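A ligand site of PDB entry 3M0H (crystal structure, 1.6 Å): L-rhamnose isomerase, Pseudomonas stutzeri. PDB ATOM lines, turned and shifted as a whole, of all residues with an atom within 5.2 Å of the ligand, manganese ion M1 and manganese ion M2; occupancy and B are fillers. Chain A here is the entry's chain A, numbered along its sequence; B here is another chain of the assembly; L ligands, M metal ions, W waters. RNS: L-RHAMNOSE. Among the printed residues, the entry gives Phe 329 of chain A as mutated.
The side-chain amino group (NZ) of Lys 221 sits close to an oxygen (O1) of the ligand (2.7 Å). A ring nitrogen (NE2) of His 101 lies within hydrogen-bond range of an oxygen (O5) of the ligand.
The side-chain carboxylate (OD1) of Asp 327 is in hydrogen-bond range of the indole nitrogen (NE1) of Trp 57 (2.9 Å). OD2 of Asp 289 lies close to NZ of Lys 221 (3.2 Å). O of Asp 289 sits at hydrogen-bond distance from NH2 of Arg 65 of chain B. The side-chain amino group of Lys 221 is in salt-bridge range of the side-chain carboxylate of Glu 224 (3.1 Å).
NE1 of Trp 57 touches C6 of the ligand, at 3.6 Å. Trp 179 touches the ligand. Phe 66 of chain B touches the ligand (CZ to O1, 3.4 Å). Hydrophobic or aromatic side chains that line the ligand: Trp 57, His 101, Trp 179, His 257, His 281 and Phe 66 of chain B. The nearest printed residue that does not touch the ligand is Phe 329 (4.1 Å).
Within 4 Å of manganese ion M1: Glu 219, Asp 254, His 257, His 281 and Asp 327.
Residues that only touch manganese ion M2: Lys 221 (3.8 Å). Four residues have an atom within 4 Å of manganese ion M2: Lys 221, Asp 254, His 257 and Asp 289.
Manganese ion M1 is bound by OD2 of Asp 327 (2.0 Å), OE2 of Glu 219 (2.1 Å), OD2 of Asp 254 (2.2 Å), O2 of the ligand (2.2 Å), ND1 of His 281 (2.2 Å) and O3 of the ligand (2.3 Å). Manganese ion M1 has six donor atoms within binding distance.
Manganese ion M2 is bound by water W3 (1.9 Å), an oxygen (O2) of the ligand (2.1 Å), water W2 (2.1 Å), a ring nitrogen (NE2) of His 257 (2.1 Å), the side-chain carboxylate of Asp 289 (2.2 Å) and an oxygen (O1) of the ligand (2.2 Å).
Water W2 lies within hydrogen-bond range of an oxygen (O4) of the ligand (2.7 Å) and the side-chain carboxylate of Asp 291 (2.7 Å). Water W3 lies within hydrogen-bond range of OD1 of Asp 291 (2.5 Å) and OD1 of Asp 254 (3.4 Å). Water W1 bridges O5 of the ligand (2.7 Å) and OD1 of Asn 127 (2.8 Å).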
ATOM      1  N   TRP A  57     -15.900  -6.097 -15.069  1.00  0.00           N
ATOM      2  CA  TRP A  57     -16.920  -5.879 -14.063  1.00  0.00           C
ATOM      3  C   TRP A  57     -17.161  -7.098 -13.167  1.00  0.00           C
ATOM      4  O   TRP A  57     -17.941  -7.038 -12.211  1.00  0.00           O
ATOM      5  CB  TRP A  57     -18.233  -5.452 -14.735  1.00  0.00           C
ATOM      6  CG  TRP A  57     -18.799  -6.451 -15.704  1.00  0.00           C
ATOM      7  CD1 TRP A  57     -19.678  -7.449 -15.425  1.00  0.00           C
ATOM      8  CD2 TRP A  57     -18.510  -6.544 -17.101  1.00  0.00           C
ATOM      9  NE1 TRP A  57     -19.981  -8.148 -16.566  1.00  0.00           N
ATOM     10  CE2 TRP A  57     -19.277  -7.615 -17.618  1.00  0.00           C
ATOM     11  CE3 TRP A  57     -17.702  -5.810 -17.976  1.00  0.00           C
ATOM     12  CZ2 TRP A  57     -19.246  -7.990 -18.964  1.00  0.00           C
ATOM     13  CZ3 TRP A  57     -17.661  -6.185 -19.320  1.00  0.00           C
ATOM     14  CH2 TRP A  57     -18.437  -7.260 -19.795  1.00  0.00           C
ATOM     15  N   HIS A 101     -15.644  -2.150 -20.103  1.00  0.00           N
ATOM     16  CA  HIS A 101     -16.964  -1.539 -20.071  1.00  0.00           C
ATOM     17  C   HIS A 101     -16.775  -0.034 -19.880  1.00  0.00           C
ATOM     18  O   HIS A 101     -16.115   0.397 -18.940  1.00  0.00           O
ATOM     19  CB  HIS A 101     -17.775  -2.129 -18.909  1.00  0.00           C
ATOM     20  CG  HIS A 101     -19.232  -2.286 -19.212  1.00  0.00           C
ATOM     21  ND1 HIS A 101     -20.055  -1.224 -19.507  1.00  0.00           N
ATOM     22  CD2 HIS A 101     -20.004  -3.405 -19.276  1.00  0.00           C
ATOM     23  CE1 HIS A 101     -21.281  -1.669 -19.749  1.00  0.00           C
ATOM     24  NE2 HIS A 101     -21.275  -2.988 -19.614  1.00  0.00           N
ATOM     25  N   TRP A 104     -17.258   2.788 -17.042  1.00  0.00           N
ATOM     26  CA  TRP A 104     -16.657   2.237 -15.829  1.00  0.00           C
ATOM     27  C   TRP A 104     -15.140   2.129 -15.913  1.00  0.00           C
ATOM     28  O   TRP A 104     -14.430   2.503 -14.982  1.00  0.00           O
ATOM     29  CB  TRP A 104     -17.206   0.842 -15.500  1.00  0.00           C
ATOM     30  CG  TRP A 104     -18.668   0.784 -15.171  1.00  0.00           C
ATOM     31  CD1 TRP A 104     -19.453   1.814 -14.728  1.00  0.00           C
ATOM     32  CD2 TRP A 104     -19.510  -0.367 -15.246  1.00  0.00           C
ATOM     33  NE1 TRP A 104     -20.733   1.372 -14.517  1.00  0.00           N
ATOM     34  CE2 TRP A 104     -20.798   0.031 -14.827  1.00  0.00           C
ATOM     35  CE3 TRP A 104     -19.308  -1.703 -15.608  1.00  0.00           C
ATOM     36  CZ2 TRP A 104     -21.881  -0.857 -14.771  1.00  0.00           C
ATOM     37  CZ3 TRP A 104     -20.379  -2.590 -15.564  1.00  0.00           C
ATOM     38  CH2 TRP A 104     -21.654  -2.157 -15.146  1.00  0.00           C
ATOM     39  N   ASN A 127     -17.725  -2.788 -24.404  1.00  0.00           N
ATOM     40  CA  ASN A 127     -19.111  -2.810 -23.947  1.00  0.00           C
ATOM     41  C   ASN A 127     -19.544  -1.386 -23.634  1.00  0.00           C
ATOM     42  O   ASN A 127     -18.903  -0.692 -22.843  1.00  0.00           O
ATOM     43  CB  ASN A 127     -19.238  -3.681 -22.692  1.00  0.00           C
ATOM     44  CG  ASN A 127     -18.980  -5.147 -22.959  1.00  0.00           C
ATOM     45  OD1 ASN A 127     -19.896  -5.898 -23.284  1.00  0.00           O
ATOM     46  ND2 ASN A 127     -17.724  -5.558 -22.842  1.00  0.00           N
ATOM     47  N   SER A 128     -20.632  -0.941 -24.256  1.00  0.00           N
ATOM     48  CA  SER A 128     -21.145   0.400 -24.019  1.00  0.00           C
ATOM     49  C   SER A 128     -22.108   0.394 -22.839  1.00  0.00           C
ATOM     50  O   SER A 128     -22.604  -0.659 -22.448  1.00  0.00           O
ATOM     51  CB  SER A 128     -21.851   0.929 -25.271  1.00  0.00           C
ATOM     52  OG  SER A 128     -22.838   0.021 -25.726  1.00  0.00           O
ATOM     53  N   PHE A 131     -27.420   2.270 -19.945  1.00  0.00           N
ATOM     54  CA  PHE A 131     -28.453   1.720 -19.081  1.00  0.00           C
ATOM     55  C   PHE A 131     -28.346   2.366 -17.703  1.00  0.00           C
ATOM     56  O   PHE A 131     -29.006   1.946 -16.741  1.00  0.00           O
ATOM     57  CB  PHE A 131     -28.325   0.181 -18.989  1.00  0.00           C
ATOM     58  CG  PHE A 131     -26.955  -0.307 -18.601  1.00  0.00           C
ATOM     59  CD1 PHE A 131     -26.536  -0.267 -17.274  1.00  0.00           C
ATOM     60  CD2 PHE A 131     -26.092  -0.844 -19.558  1.00  0.00           C
ATOM     61  CE1 PHE A 131     -25.285  -0.757 -16.904  1.00  0.00           C
ATOM     62  CE2 PHE A 131     -24.840  -1.341 -19.196  1.00  0.00           C
ATOM     63  CZ  PHE A 131     -24.431  -1.301 -17.872  1.00  0.00           C
ATOM     64  N   TRP A 179     -25.678  -3.800 -25.122  1.00  0.00           N
ATOM     65  CA  TRP A 179     -26.785  -4.306 -24.335  1.00  0.00           C
ATOM     66  C   TRP A 179     -27.375  -3.075 -23.659  1.00  0.00           C
ATOM     67  O   TRP A 179     -26.656  -2.305 -23.025  1.00  0.00           O
ATOM     68  CB  TRP A 179     -26.362  -5.283 -23.240  1.00  0.00           C
ATOM     69  CG  TRP A 179     -27.547  -5.599 -22.337  1.00  0.00           C
ATOM     70  CD1 TRP A 179     -28.629  -6.368 -22.649  1.00  0.00           C
ATOM     71  CD2 TRP A 179     -27.823  -5.020 -21.048  1.00  0.00           C
ATOM     72  NE1 TRP A 179     -29.573  -6.301 -21.647  1.00  0.00           N
ATOM     73  CE2 TRP A 179     -29.099  -5.479 -20.663  1.00  0.00           C
ATOM     74  CE3 TRP A 179     -27.124  -4.149 -20.200  1.00  0.00           C
ATOM     75  CZ2 TRP A 179     -29.696  -5.099 -19.445  1.00  0.00           C
ATOM     76  CZ3 TRP A 179     -27.709  -3.782 -18.994  1.00  0.00           C
ATOM     77  CH2 TRP A 179     -28.983  -4.254 -18.625  1.00  0.00           C
ATOM     78  N   GLU A 219     -27.092  -7.724 -27.821  1.00  0.00           N
ATOM     79  CA  GLU A 219     -27.430  -8.738 -26.812  1.00  0.00           C
ATOM     80  C   GLU A 219     -28.883  -8.666 -26.354  1.00  0.00           C
ATOM     81  O   GLU A 219     -29.303  -7.681 -25.757  1.00  0.00           O
ATOM     82  CB  GLU A 219     -26.486  -8.571 -25.624  1.00  0.00           C
ATOM     83  CG  GLU A 219     -26.707  -9.537 -24.477  1.00  0.00           C
ATOM     84  CD  GLU A 219     -25.752  -9.310 -23.325  1.00  0.00           C
ATOM     85  OE1 GLU A 219     -25.022  -8.290 -23.328  1.00  0.00           O
ATOM     86  OE2 GLU A 219     -25.726 -10.147 -22.404  1.00  0.00           O
ATOM     87  N   LYS A 221     -32.342  -9.774 -24.183  1.00  0.00           N
ATOM     88  CA  LYS A 221     -32.648 -10.099 -22.789  1.00  0.00           C
ATOM     89  C   LYS A 221     -34.157  -9.995 -22.595  1.00  0.00           C
ATOM     90  O   LYS A 221     -34.761  -8.978 -22.919  1.00  0.00           O
ATOM     91  CB  LYS A 221     -31.925  -9.144 -21.849  1.00  0.00           C
ATOM     92  CG  LYS A 221     -31.953  -9.596 -20.392  1.00  0.00           C
ATOM     93  CD  LYS A 221     -31.212  -8.645 -19.485  1.00  0.00           C
ATOM     94  CE  LYS A 221     -31.176  -9.180 -18.064  1.00  0.00           C
ATOM     95  NZ  LYS A 221     -30.525  -8.217 -17.117  1.00  0.00           N
ATOM     96  N   GLU A 224     -35.600  -7.209 -17.236  1.00  0.00           N
ATOM     97  CA  GLU A 224     -34.672  -6.602 -16.268  1.00  0.00           C
ATOM     98  C   GLU A 224     -33.602  -5.801 -17.008  1.00  0.00           C
ATOM     99  O   GLU A 224     -32.773  -6.361 -17.714  1.00  0.00           O
ATOM    100  CB  GLU A 224     -33.987  -7.646 -15.362  1.00  0.00           C
ATOM    101  CG  GLU A 224     -33.117  -6.961 -14.298  1.00  0.00           C
ATOM    102  CD  GLU A 224     -32.110  -7.877 -13.632  1.00  0.00           C
ATOM    103  OE1 GLU A 224     -31.603  -8.803 -14.292  1.00  0.00           O
ATOM    104  OE2 GLU A 224     -31.808  -7.645 -12.437  1.00  0.00           O
ATOM    105  N   LEU A 252     -25.431 -11.715 -29.840  1.00  0.00           N
ATOM    106  CA  LEU A 252     -24.702 -12.262 -28.701  1.00  0.00           C
ATOM    107  C   LEU A 252     -25.710 -12.953 -27.793  1.00  0.00           C
ATOM    108  O   LEU A 252     -26.756 -12.381 -27.467  1.00  0.00           O
ATOM    109  CB  LEU A 252     -23.963 -11.149 -27.947  1.00  0.00           C
ATOM    110  CG  LEU A 252     -23.067 -11.643 -26.812  1.00  0.00           C
ATOM    111  CD1 LEU A 252     -21.759 -10.874 -26.793  1.00  0.00           C
ATOM    112  CD2 LEU A 252     -23.808 -11.518 -25.494  1.00  0.00           C
ATOM    113  N   ASP A 254     -26.481 -14.553 -24.206  1.00  0.00           N
ATOM    114  CA  ASP A 254     -26.125 -14.598 -22.791  1.00  0.00           C
ATOM    115  C   ASP A 254     -27.035 -15.691 -22.238  1.00  0.00           C
ATOM    116  O   ASP A 254     -28.252 -15.567 -22.262  1.00  0.00           O
ATOM    117  CB  ASP A 254     -26.411 -13.253 -22.120  1.00  0.00           C
ATOM    118  CG  ASP A 254     -25.978 -13.218 -20.668  1.00  0.00           C
ATOM    119  OD1 ASP A 254     -26.369 -14.135 -19.923  1.00  0.00           O
ATOM    120  OD2 ASP A 254     -25.255 -12.285 -20.267  1.00  0.00           O
ATOM    121  N   HIS A 257     -30.372 -15.048 -20.138  1.00  0.00           N
ATOM    122  CA  HIS A 257     -31.338 -14.076 -20.645  1.00  0.00           C
ATOM    123  C   HIS A 257     -32.565 -14.636 -21.347  1.00  0.00           C
ATOM    124  O   HIS A 257     -33.220 -13.945 -22.131  1.00  0.00           O
ATOM    125  CB  HIS A 257     -30.635 -13.112 -21.602  1.00  0.00           C
ATOM    126  CG  HIS A 257     -29.662 -12.195 -20.931  1.00  0.00           C
ATOM    127  ND1 HIS A 257     -29.102 -11.113 -21.575  1.00  0.00           N
ATOM    128  CD2 HIS A 257     -29.168 -12.179 -19.678  1.00  0.00           C
ATOM    129  CE1 HIS A 257     -28.308 -10.470 -20.741  1.00  0.00           C
ATOM    130  NE2 HIS A 257     -28.323 -11.101 -19.579  1.00  0.00           N
ATOM    131  N   HIS A 281     -22.077 -15.003 -23.790  1.00  0.00           N
ATOM    132  CA  HIS A 281     -21.846 -14.411 -22.479  1.00  0.00           C
ATOM    133  C   HIS A 281     -22.186 -15.605 -21.594  1.00  0.00           C
ATOM    134  O   HIS A 281     -23.360 -15.954 -21.432  1.00  0.00           O
ATOM    135  CB  HIS A 281     -22.784 -13.249 -22.202  1.00  0.00           C
ATOM    136  CG  HIS A 281     -22.190 -11.900 -22.511  1.00  0.00           C
ATOM    137  ND1 HIS A 281     -22.759 -10.724 -22.089  1.00  0.00           N
ATOM    138  CD2 HIS A 281     -21.071 -11.559 -23.193  1.00  0.00           C
ATOM    139  CE1 HIS A 281     -22.024  -9.703 -22.505  1.00  0.00           C
ATOM    140  NE2 HIS A 281     -20.994 -10.185 -23.175  1.00  0.00           N
ATOM    141  N   ASP A 289     -31.845 -13.903 -14.535  1.00  0.00           N
ATOM    142  CA  ASP A 289     -30.495 -13.615 -15.013  1.00  0.00           C
ATOM    143  C   ASP A 289     -29.628 -13.543 -13.769  1.00  0.00           C
ATOM    144  O   ASP A 289     -29.107 -12.489 -13.401  1.00  0.00           O
ATOM    145  CB  ASP A 289     -30.472 -12.289 -15.772  1.00  0.00           C
ATOM    146  CG  ASP A 289     -29.131 -11.978 -16.351  1.00  0.00           C
ATOM    147  OD1 ASP A 289     -28.396 -12.938 -16.690  1.00  0.00           O
ATOM    148  OD2 ASP A 289     -28.797 -10.775 -16.474  1.00  0.00           O
ATOM    149  N   ASP A 291     -26.658 -14.618 -13.133  1.00  0.00           N
ATOM    150  CA  ASP A 291     -25.232 -14.336 -13.342  1.00  0.00           C
ATOM    151  C   ASP A 291     -24.291 -15.116 -12.431  1.00  0.00           C
ATOM    152  O   ASP A 291     -23.271 -14.587 -11.965  1.00  0.00           O
ATOM    153  CB  ASP A 291     -24.961 -12.836 -13.199  1.00  0.00           C
ATOM    154  CG  ASP A 291     -25.408 -12.046 -14.416  1.00  0.00           C
ATOM    155  OD1 ASP A 291     -25.152 -12.525 -15.542  1.00  0.00           O
ATOM    156  OD2 ASP A 291     -25.999 -10.954 -14.246  1.00  0.00           O
ATOM    157  N   ASP A 327     -19.770 -13.467 -18.428  1.00  0.00           N
ATOM    158  CA  ASP A 327     -20.507 -12.307 -17.942  1.00  0.00           C
ATOM    159  C   ASP A 327     -21.163 -12.790 -16.672  1.00  0.00           C
ATOM    160  O   ASP A 327     -22.245 -13.385 -16.707  1.00  0.00           O
ATOM    161  CB  ASP A 327     -21.569 -11.836 -18.926  1.00  0.00           C
ATOM    162  CG  ASP A 327     -22.352 -10.636 -18.403  1.00  0.00           C
ATOM    163  OD1 ASP A 327     -21.971 -10.103 -17.332  1.00  0.00           O
ATOM    164  OD2 ASP A 327     -23.336 -10.227 -19.042  1.00  0.00           O
ATOM    165  N   PHE A 329     -21.474 -12.033 -12.103  1.00  0.00           N
ATOM    166  CA  PHE A 329     -21.327 -11.146 -10.965  1.00  0.00           C
ATOM    167  C   PHE A 329     -21.144 -12.082  -9.787  1.00  0.00           C
ATOM    168  O   PHE A 329     -21.858 -13.084  -9.662  1.00  0.00           O
ATOM    169  CB  PHE A 329     -22.561 -10.258 -10.796  1.00  0.00           C
ATOM    170  CG  PHE A 329     -22.606  -9.111 -11.760  1.00  0.00           C
ATOM    171  CD1 PHE A 329     -21.764  -8.017 -11.595  1.00  0.00           C
ATOM    172  CD2 PHE A 329     -23.450  -9.153 -12.865  1.00  0.00           C
ATOM    173  CE1 PHE A 329     -21.771  -6.974 -12.516  1.00  0.00           C
ATOM    174  CE2 PHE A 329     -23.457  -8.110 -13.785  1.00  0.00           C
ATOM    175  CZ  PHE A 329     -22.617  -7.024 -13.615  1.00  0.00           C
ATOM    176  N   ARG B  65     -30.728  -3.337  -9.965  1.00  0.00           N
ATOM    177  CA  ARG B  65     -29.301  -3.462  -9.678  1.00  0.00           C
ATOM    178  C   ARG B  65     -28.467  -2.727 -10.722  1.00  0.00           C
ATOM    179  O   ARG B  65     -27.284  -2.477 -10.506  1.00  0.00           O
ATOM    180  CB  ARG B  65     -28.874  -4.926  -9.626  1.00  0.00           C
ATOM    181  CG  ARG B  65     -29.154  -5.706 -10.892  1.00  0.00           C
ATOM    182  CD  ARG B  65     -28.527  -7.095 -10.855  1.00  0.00           C
ATOM    183  NE  ARG B  65     -28.989  -7.897 -11.988  1.00  0.00           N
ATOM    184  CZ  ARG B  65     -28.252  -8.777 -12.660  1.00  0.00           C
ATOM    185  NH1 ARG B  65     -26.983  -8.995 -12.321  1.00  0.00           N
ATOM    186  NH2 ARG B  65     -28.781  -9.424 -13.685  1.00  0.00           N
ATOM    187  N   PHE B  66     -29.086  -2.369 -11.839  1.00  0.00           N
ATOM    188  CA  PHE B  66     -28.381  -1.670 -12.913  1.00  0.00           C
ATOM    189  C   PHE B  66     -28.365  -0.142 -12.771  1.00  0.00           C
ATOM    190  O   PHE B  66     -27.393   0.496 -13.176  1.00  0.00           O
ATOM    191  CB  PHE B  66     -28.982  -2.036 -14.270  1.00  0.00           C
ATOM    192  CG  PHE B  66     -28.722  -3.447 -14.676  1.00  0.00           C
ATOM    193  CD1 PHE B  66     -27.453  -3.837 -15.106  1.00  0.00           C
ATOM    194  CD2 PHE B  66     -29.725  -4.412 -14.581  1.00  0.00           C
ATOM    195  CE1 PHE B  66     -27.185  -5.163 -15.439  1.00  0.00           C
ATOM    196  CE2 PHE B  66     -29.469  -5.745 -14.909  1.00  0.00           C
ATOM    197  CZ  PHE B  66     -28.197  -6.113 -15.344  1.00  0.00           C
HETATM  198  C1  RNS L   1     -27.151  -7.329 -18.730  1.00  0.00           C
HETATM  199  C2  RNS L   1     -26.258  -8.002 -19.765  1.00  0.00           C
HETATM  200  C3  RNS L   1     -24.973  -7.205 -19.974  1.00  0.00           C
HETATM  201  C4  RNS L   1     -24.310  -6.780 -18.657  1.00  0.00           C
HETATM  202  C5  RNS L   1     -22.935  -6.183 -18.943  1.00  0.00           C
HETATM  203  C6  RNS L   1     -22.328  -5.678 -17.638  1.00  0.00           C
HETATM  204  O1  RNS L   1     -28.025  -7.984 -18.160  1.00  0.00           O
HETATM  205  O2  RNS L   1     -25.954  -9.319 -19.342  1.00  0.00           O
HETATM  206  O3  RNS L   1     -24.067  -7.980 -20.747  1.00  0.00           O
HETATM  207  O4  RNS L   1     -24.184  -7.899 -17.783  1.00  0.00           O
HETATM  208  O5  RNS L   1     -23.066  -5.103 -19.851  1.00  0.00           O
HETATM  209 MN    MN M   1     -24.464 -10.276 -20.695  1.00  0.00          MN
HETATM  210 MN    MN M   2     -27.347 -10.091 -17.978  1.00  0.00          MN
HETATM  211  O   HOH W   1     -22.565  -5.432 -22.457  1.00  0.00           O
HETATM  212  O   HOH W   2     -26.089  -9.323 -16.454  1.00  0.00           O
HETATM  213  O   HOH W   3     -26.540 -11.767 -17.493  1.00  0.00           O
